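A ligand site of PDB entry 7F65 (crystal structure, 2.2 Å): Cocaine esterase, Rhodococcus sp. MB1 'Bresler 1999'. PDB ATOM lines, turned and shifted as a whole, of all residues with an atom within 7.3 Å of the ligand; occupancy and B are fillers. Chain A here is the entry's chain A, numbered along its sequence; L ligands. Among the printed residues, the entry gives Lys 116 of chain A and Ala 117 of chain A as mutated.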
ATOM      1  N   PRO A  43      -7.916 -24.406 -31.230  1.00  0.00           N
ATOM      2  CA  PRO A  43      -8.892 -25.346 -31.774  1.00  0.00           C
ATOM      3  C   PRO A  43      -9.326 -25.041 -33.191  1.00  0.00           C
ATOM      4  O   PRO A  43     -10.215 -25.724 -33.702  1.00  0.00           O
ATOM      5  CB  PRO A  43     -10.074 -25.178 -30.804  1.00  0.00           C
ATOM      6  CG  PRO A  43     -10.017 -23.718 -30.470  1.00  0.00           C
ATOM      7  CD  PRO A  43      -8.557 -23.344 -30.436  1.00  0.00           C
ATOM      8  N   TYR A  44      -8.760 -24.014 -33.827  1.00  0.00           N
ATOM      9  CA  TYR A  44      -9.242 -23.540 -35.124  1.00  0.00           C
ATOM     10  C   TYR A  44      -8.193 -23.734 -36.227  1.00  0.00           C
ATOM     11  O   TYR A  44      -8.128 -22.921 -37.158  1.00  0.00           O
ATOM     12  CB  TYR A  44      -9.658 -22.072 -35.031  1.00  0.00           C
ATOM     13  CG  TYR A  44     -10.556 -21.735 -33.863  1.00  0.00           C
ATOM     14  CD1 TYR A  44     -11.826 -22.299 -33.739  1.00  0.00           C
ATOM     15  CD2 TYR A  44     -10.139 -20.826 -32.886  1.00  0.00           C
ATOM     16  CE1 TYR A  44     -12.648 -21.982 -32.671  1.00  0.00           C
ATOM     17  CE2 TYR A  44     -10.958 -20.505 -31.826  1.00  0.00           C
ATOM     18  CZ  TYR A  44     -12.202 -21.084 -31.716  1.00  0.00           C
ATOM     19  OH  TYR A  44     -13.014 -20.765 -30.668  1.00  0.00           O
ATOM     20  N   HIS A  87     -12.847 -27.875 -23.541  1.00  0.00           N
ATOM     21  CA  HIS A  87     -12.358 -27.550 -22.204  1.00  0.00           C
ATOM     22  C   HIS A  87     -11.818 -28.728 -21.406  1.00  0.00           C
ATOM     23  O   HIS A  87     -10.823 -28.573 -20.698  1.00  0.00           O
ATOM     24  CB  HIS A  87     -13.451 -26.881 -21.350  1.00  0.00           C
ATOM     25  CG  HIS A  87     -14.109 -25.704 -22.002  1.00  0.00           C
ATOM     26  ND1 HIS A  87     -13.421 -24.793 -22.773  1.00  0.00           N
ATOM     27  CD2 HIS A  87     -15.401 -25.292 -21.992  1.00  0.00           C
ATOM     28  CE1 HIS A  87     -14.263 -23.871 -23.204  1.00  0.00           C
ATOM     29  NE2 HIS A  87     -15.467 -24.146 -22.749  1.00  0.00           N
ATOM     30  N   LYS A 116      -6.119 -15.416 -27.941  1.00  0.00           N
ATOM     31  CA  LYS A 116      -7.372 -14.755 -27.635  1.00  0.00           C
ATOM     32  C   LYS A 116      -8.520 -15.754 -27.471  1.00  0.00           C
ATOM     33  O   LYS A 116      -8.580 -16.776 -28.164  1.00  0.00           O
ATOM     34  CB  LYS A 116      -7.704 -13.747 -28.750  1.00  0.00           C
ATOM     35  CG  LYS A 116      -9.050 -13.041 -28.653  1.00  0.00           C
ATOM     36  CD  LYS A 116      -9.179 -12.012 -29.776  1.00  0.00           C
ATOM     37  CE  LYS A 116     -10.491 -11.208 -29.679  1.00  0.00           C
ATOM     38  NZ  LYS A 116     -11.713 -12.013 -29.967  1.00  0.00           N
ATOM     39  N   ALA A 117      -9.448 -15.436 -26.559  1.00  0.00           N
ATOM     40  CA  ALA A 117     -10.711 -16.155 -26.360  1.00  0.00           C
ATOM     41  C   ALA A 117     -10.419 -17.600 -25.972  1.00  0.00           C
ATOM     42  O   ALA A 117      -9.804 -17.820 -24.912  1.00  0.00           O
ATOM     43  CB  ALA A 117     -11.576 -15.969 -27.619  1.00  0.00           C
ATOM     44  N   TYR A 118     -10.822 -18.612 -26.753  1.00  0.00           N
ATOM     45  CA  TYR A 118     -10.470 -19.986 -26.411  1.00  0.00           C
ATOM     46  C   TYR A 118      -8.957 -20.170 -26.303  1.00  0.00           C
ATOM     47  O   TYR A 118      -8.472 -20.913 -25.449  1.00  0.00           O
ATOM     48  CB  TYR A 118     -11.062 -20.937 -27.458  1.00  0.00           C
ATOM     49  CG  TYR A 118     -11.164 -22.389 -27.051  1.00  0.00           C
ATOM     50  CD1 TYR A 118     -10.041 -23.201 -27.002  1.00  0.00           C
ATOM     51  CD2 TYR A 118     -12.401 -22.947 -26.752  1.00  0.00           C
ATOM     52  CE1 TYR A 118     -10.153 -24.546 -26.652  1.00  0.00           C
ATOM     53  CE2 TYR A 118     -12.524 -24.276 -26.394  1.00  0.00           C
ATOM     54  CZ  TYR A 118     -11.395 -25.071 -26.346  1.00  0.00           C
ATOM     55  OH  TYR A 118     -11.528 -26.390 -25.997  1.00  0.00           O
ATOM     56  N   LEU A 119      -8.186 -19.465 -27.144  1.00  0.00           N
ATOM     57  CA  LEU A 119      -6.738 -19.492 -27.028  1.00  0.00           C
ATOM     58  C   LEU A 119      -6.229 -18.733 -25.811  1.00  0.00           C
ATOM     59  O   LEU A 119      -5.057 -18.883 -25.443  1.00  0.00           O
ATOM     60  CB  LEU A 119      -6.098 -18.947 -28.323  1.00  0.00           C
ATOM     61  CG  LEU A 119      -6.186 -19.769 -29.621  1.00  0.00           C
ATOM     62  CD1 LEU A 119      -7.608 -19.897 -30.149  1.00  0.00           C
ATOM     63  CD2 LEU A 119      -5.314 -19.130 -30.683  1.00  0.00           C
ATOM     64  N   GLY A 120      -7.079 -17.940 -25.170  1.00  0.00           N
ATOM     65  CA  GLY A 120      -6.724 -17.365 -23.875  1.00  0.00           C
ATOM     66  C   GLY A 120      -7.128 -18.298 -22.733  1.00  0.00           C
ATOM     67  O   GLY A 120      -6.396 -18.437 -21.744  1.00  0.00           O
ATOM     68  N   VAL A 121      -8.300 -18.920 -22.849  1.00  0.00           N
ATOM     69  CA  VAL A 121      -8.737 -19.877 -21.845  1.00  0.00           C
ATOM     70  C   VAL A 121      -7.708 -20.987 -21.661  1.00  0.00           C
ATOM     71  O   VAL A 121      -7.371 -21.360 -20.541  1.00  0.00           O
ATOM     72  CB  VAL A 121     -10.122 -20.435 -22.208  1.00  0.00           C
ATOM     73  CG1 VAL A 121     -10.460 -21.648 -21.313  1.00  0.00           C
ATOM     74  CG2 VAL A 121     -11.175 -19.361 -22.089  1.00  0.00           C
ATOM     75  N   MET A 141      -8.794 -11.238 -23.945  1.00  0.00           N
ATOM     76  CA  MET A 141     -10.255 -11.268 -24.040  1.00  0.00           C
ATOM     77  C   MET A 141     -10.776 -12.683 -23.777  1.00  0.00           C
ATOM     78  O   MET A 141     -11.436 -13.305 -24.607  1.00  0.00           O
ATOM     79  CB  MET A 141     -10.713 -10.716 -25.391  1.00  0.00           C
ATOM     80  CG  MET A 141     -10.085  -9.345 -25.686  1.00  0.00           C
ATOM     81  SD  MET A 141     -10.608  -8.476 -27.160  1.00  0.00           S
ATOM     82  CE  MET A 141      -9.046  -8.362 -27.989  1.00  0.00           C
ATOM     83  N   LEU A 146     -15.606 -20.812 -16.953  1.00  0.00           N
ATOM     84  CA  LEU A 146     -16.349 -20.999 -18.193  1.00  0.00           C
ATOM     85  C   LEU A 146     -17.856 -20.837 -18.018  1.00  0.00           C
ATOM     86  O   LEU A 146     -18.543 -20.524 -18.992  1.00  0.00           O
ATOM     87  CB  LEU A 146     -16.054 -22.380 -18.798  1.00  0.00           C
ATOM     88  CG  LEU A 146     -14.700 -22.542 -19.476  1.00  0.00           C
ATOM     89  CD1 LEU A 146     -14.409 -21.362 -20.395  1.00  0.00           C
ATOM     90  CD2 LEU A 146     -13.578 -22.745 -18.467  1.00  0.00           C
ATOM     91  N   ALA A 149     -18.171 -16.882 -18.009  1.00  0.00           N
ATOM     92  CA  ALA A 149     -18.023 -16.458 -19.400  1.00  0.00           C
ATOM     93  C   ALA A 149     -17.271 -17.558 -20.148  1.00  0.00           C
ATOM     94  O   ALA A 149     -16.233 -18.023 -19.692  1.00  0.00           O
ATOM     95  CB  ALA A 149     -17.279 -15.103 -19.522  1.00  0.00           C
ATOM     96  N   PRO A 150     -17.789 -17.966 -21.312  1.00  0.00           N
ATOM     97  CA  PRO A 150     -18.868 -17.296 -22.030  1.00  0.00           C
ATOM     98  C   PRO A 150     -20.214 -18.028 -22.063  1.00  0.00           C
ATOM     99  O   PRO A 150     -21.091 -17.576 -22.796  1.00  0.00           O
ATOM    100  CB  PRO A 150     -18.313 -17.235 -23.442  1.00  0.00           C
ATOM    101  CG  PRO A 150     -17.645 -18.596 -23.584  1.00  0.00           C
ATOM    102  CD  PRO A 150     -17.111 -18.942 -22.187  1.00  0.00           C
ATOM    103  N   TRP A 151     -20.383 -19.115 -21.317  1.00  0.00           N
ATOM    104  CA  TRP A 151     -21.585 -19.922 -21.575  1.00  0.00           C
ATOM    105  C   TRP A 151     -22.795 -19.505 -20.748  1.00  0.00           C
ATOM    106  O   TRP A 151     -23.919 -19.535 -21.268  1.00  0.00           O
ATOM    107  CB  TRP A 151     -21.276 -21.414 -21.397  1.00  0.00           C
ATOM    108  CG  TRP A 151     -20.096 -21.870 -22.209  1.00  0.00           C
ATOM    109  CD1 TRP A 151     -19.021 -22.574 -21.761  1.00  0.00           C
ATOM    110  CD2 TRP A 151     -19.857 -21.637 -23.609  1.00  0.00           C
ATOM    111  NE1 TRP A 151     -18.134 -22.797 -22.773  1.00  0.00           N
ATOM    112  CE2 TRP A 151     -18.620 -22.236 -23.930  1.00  0.00           C
ATOM    113  CE3 TRP A 151     -20.574 -20.971 -24.622  1.00  0.00           C
ATOM    114  CZ2 TRP A 151     -18.074 -22.192 -25.207  1.00  0.00           C
ATOM    115  CZ3 TRP A 151     -20.034 -20.942 -25.900  1.00  0.00           C
ATOM    116  CH2 TRP A 151     -18.792 -21.543 -26.183  1.00  0.00           C
ATOM    117  N   ALA A 162     -24.360 -17.038 -27.660  1.00  0.00           N
ATOM    118  CA  ALA A 162     -22.961 -17.445 -27.584  1.00  0.00           C
ATOM    119  C   ALA A 162     -22.828 -18.942 -27.821  1.00  0.00           C
ATOM    120  O   ALA A 162     -21.954 -19.394 -28.566  1.00  0.00           O
ATOM    121  CB  ALA A 162     -22.373 -17.070 -26.220  1.00  0.00           C
ATOM    122  N   LEU A 163     -23.702 -19.732 -27.189  1.00  0.00           N
ATOM    123  CA  LEU A 163     -23.623 -21.179 -27.301  1.00  0.00           C
ATOM    124  C   LEU A 163     -23.900 -21.646 -28.724  1.00  0.00           C
ATOM    125  O   LEU A 163     -23.121 -22.396 -29.310  1.00  0.00           O
ATOM    126  CB  LEU A 163     -24.609 -21.821 -26.337  1.00  0.00           C
ATOM    127  CG  LEU A 163     -24.642 -23.358 -26.382  1.00  0.00           C
ATOM    128  CD1 LEU A 163     -23.267 -23.917 -26.029  1.00  0.00           C
ATOM    129  CD2 LEU A 163     -25.704 -23.906 -25.455  1.00  0.00           C
ATOM    130  N   GLY A 165     -24.058 -19.971 -31.593  1.00  0.00           N
ATOM    131  CA  GLY A 165     -23.162 -19.444 -32.598  1.00  0.00           C
ATOM    132  C   GLY A 165     -21.818 -20.156 -32.600  1.00  0.00           C
ATOM    133  O   GLY A 165     -21.338 -20.585 -33.651  1.00  0.00           O
ATOM    134  N   TRP A 166     -21.201 -20.298 -31.427  1.00  0.00           N
ATOM    135  CA  TRP A 166     -19.927 -21.003 -31.374  1.00  0.00           C
ATOM    136  C   TRP A 166     -20.076 -22.455 -31.831  1.00  0.00           C
ATOM    137  O   TRP A 166     -19.249 -22.945 -32.615  1.00  0.00           O
ATOM    138  CB  TRP A 166     -19.333 -20.942 -29.978  1.00  0.00           C
ATOM    139  CG  TRP A 166     -17.918 -21.459 -29.919  1.00  0.00           C
ATOM    140  CD1 TRP A 166     -16.794 -20.837 -30.383  1.00  0.00           C
ATOM    141  CD2 TRP A 166     -17.483 -22.691 -29.348  1.00  0.00           C
ATOM    142  NE1 TRP A 166     -15.692 -21.599 -30.137  1.00  0.00           N
ATOM    143  CE2 TRP A 166     -16.077 -22.751 -29.501  1.00  0.00           C
ATOM    144  CE3 TRP A 166     -18.138 -23.754 -28.702  1.00  0.00           C
ATOM    145  CZ2 TRP A 166     -15.321 -23.827 -29.049  1.00  0.00           C
ATOM    146  CZ3 TRP A 166     -17.380 -24.825 -28.258  1.00  0.00           C
ATOM    147  CH2 TRP A 166     -15.990 -24.854 -28.445  1.00  0.00           C
ATOM    148  N   LEU A 169     -20.120 -22.757 -35.562  1.00  0.00           N
ATOM    149  CA  LEU A 169     -18.823 -22.563 -36.212  1.00  0.00           C
ATOM    150  C   LEU A 169     -17.946 -23.790 -36.042  1.00  0.00           C
ATOM    151  O   LEU A 169     -17.223 -24.182 -36.968  1.00  0.00           O
ATOM    152  CB  LEU A 169     -18.120 -21.331 -35.663  1.00  0.00           C
ATOM    153  CG  LEU A 169     -18.752 -19.975 -35.969  1.00  0.00           C
ATOM    154  CD1 LEU A 169     -18.386 -18.957 -34.912  1.00  0.00           C
ATOM    155  CD2 LEU A 169     -18.367 -19.475 -37.360  1.00  0.00           C
ATOM    156  N   PHE A 261     -16.283 -11.757 -22.944  1.00  0.00           N
ATOM    157  CA  PHE A 261     -15.494 -12.253 -21.811  1.00  0.00           C
ATOM    158  C   PHE A 261     -15.125 -11.175 -20.801  1.00  0.00           C
ATOM    159  O   PHE A 261     -14.440 -11.493 -19.819  1.00  0.00           O
ATOM    160  CB  PHE A 261     -14.185 -12.908 -22.305  1.00  0.00           C
ATOM    161  CG  PHE A 261     -14.376 -14.092 -23.193  1.00  0.00           C
ATOM    162  CD1 PHE A 261     -14.693 -13.927 -24.528  1.00  0.00           C
ATOM    163  CD2 PHE A 261     -14.258 -15.384 -22.687  1.00  0.00           C
ATOM    164  CE1 PHE A 261     -14.877 -15.010 -25.348  1.00  0.00           C
ATOM    165  CE2 PHE A 261     -14.434 -16.464 -23.502  1.00  0.00           C
ATOM    166  CZ  PHE A 261     -14.751 -16.281 -24.850  1.00  0.00           C
ATOM    167  N   HIS A 287     -16.100  -8.922 -29.514  1.00  0.00           N
ATOM    168  CA  HIS A 287     -15.305 -10.119 -29.756  1.00  0.00           C
ATOM    169  C   HIS A 287     -14.864 -10.202 -31.211  1.00  0.00           C
ATOM    170  O   HIS A 287     -13.730 -10.594 -31.491  1.00  0.00           O
ATOM    171  CB  HIS A 287     -16.118 -11.352 -29.380  1.00  0.00           C
ATOM    172  CG  HIS A 287     -15.595 -12.636 -29.960  1.00  0.00           C
ATOM    173  ND1 HIS A 287     -16.005 -13.112 -31.185  1.00  0.00           N
ATOM    174  CD2 HIS A 287     -14.733 -13.547 -29.467  1.00  0.00           C
ATOM    175  CE1 HIS A 287     -15.407 -14.270 -31.427  1.00  0.00           C
ATOM    176  NE2 HIS A 287     -14.624 -14.555 -30.406  1.00  0.00           N
ATOM    177  N   LEU A 407     -21.925 -11.966 -28.911  1.00  0.00           N
ATOM    178  CA  LEU A 407     -20.781 -12.630 -29.536  1.00  0.00           C
ATOM    179  C   LEU A 407     -21.012 -12.874 -31.023  1.00  0.00           C
ATOM    180  O   LEU A 407     -20.225 -12.426 -31.866  1.00  0.00           O
ATOM    181  CB  LEU A 407     -20.465 -13.955 -28.842  1.00  0.00           C
ATOM    182  CG  LEU A 407     -19.819 -13.814 -27.464  1.00  0.00           C
ATOM    183  CD1 LEU A 407     -19.440 -15.180 -26.875  1.00  0.00           C
ATOM    184  CD2 LEU A 407     -18.596 -12.910 -27.568  1.00  0.00           C
ATOM    185  N   PHE A 408     -22.080 -13.580 -31.371  1.00  0.00           N
ATOM    186  CA  PHE A 408     -22.322 -13.998 -32.739  1.00  0.00           C
ATOM    187  C   PHE A 408     -23.609 -13.463 -33.339  1.00  0.00           C
ATOM    188  O   PHE A 408     -23.668 -13.285 -34.560  1.00  0.00           O
ATOM    189  CB  PHE A 408     -22.330 -15.532 -32.810  1.00  0.00           C
ATOM    190  CG  PHE A 408     -21.080 -16.145 -32.262  1.00  0.00           C
ATOM    191  CD1 PHE A 408     -19.885 -16.012 -32.947  1.00  0.00           C
ATOM    192  CD2 PHE A 408     -21.093 -16.805 -31.055  1.00  0.00           C
ATOM    193  CE1 PHE A 408     -18.713 -16.555 -32.438  1.00  0.00           C
ATOM    194  CE2 PHE A 408     -19.928 -17.346 -30.535  1.00  0.00           C
ATOM    195  CZ  PHE A 408     -18.744 -17.228 -31.233  1.00  0.00           C
HETATM  196  C1  LIG L   1     -13.407 -17.980 -29.457  1.00  0.00           C
HETATM  197  O1  LIG L   1     -13.448 -17.093 -30.337  1.00  0.00           O
HETATM  198  O2  LIG L   1     -12.367 -18.659 -29.287  1.00  0.00           O
HETATM  199  C2  LIG L   1     -14.611 -18.208 -28.627  1.00  0.00           C
HETATM  200  C3  LIG L   1     -15.706 -17.363 -28.793  1.00  0.00           C
HETATM  201  C4  LIG L   1     -16.845 -17.571 -28.027  1.00  0.00           C
HETATM  202  C5  LIG L   1     -16.881 -18.626 -27.108  1.00  0.00           C
HETATM  203  C6  LIG L   1     -15.781 -19.461 -26.959  1.00  0.00           C
HETATM  204  C7  LIG L   1     -14.650 -19.250 -27.712  1.00  0.00           C
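The indole nitrogen (NE1) of Trp 166 sits at hydrogen-bond distance from the side-chain hydroxyl (OH) of Tyr 44, 2.9 Å away. The side-chain amino group (NZ) of Lys 116 sits at hydrogen-bond distance from the backbone carbonyl oxygen (O) of His 287. N of His 87 lies within hydrogen-bond range of OH of Tyr 118 (3.2 Å). NE1 of Trp 151 sits at hydrogen-bond distance from NE2 of His 87 (3.0 Å). The backbone NH (N) of Trp 151 is in hydrogen-bond range of the backbone carbonyl oxygen (O) of Leu 146 (3.3 Å).
Ala 117 touches the ligand (CB to O2, 3.3 Å). Pro 150 touches the ligand (CG to C5, 3.6 Å). CH2 of Trp 151 touches C5 of the ligand, at 3.6 Å. NE1 of Trp 166 touches C7 of the ligand (3.5 Å). CZ of Phe 261 touches C5 of the ligand (3.9 Å). Leu 407 touches the ligand (CD1 to C4, 3.7 Å). Phe 408 touches the ligand. Hydrophobic or aromatic side chains that line the ligand: Tyr 44, Ala 117, Tyr 118, Pro 150, Trp 151, Trp 166, Phe 261, His 287, Leu 407 and Phe 408.
OH of Tyr 44 lies within hydrogen-bond range of O2 of the ligand (2.6 Å). A ring nitrogen (NE2) of His 287 is in hydrogen-bond range of an oxygen (O1) of the ligand. The backbone NH of Tyr 118 lies within hydrogen-bond range of an oxygen (O2) of the ligand.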
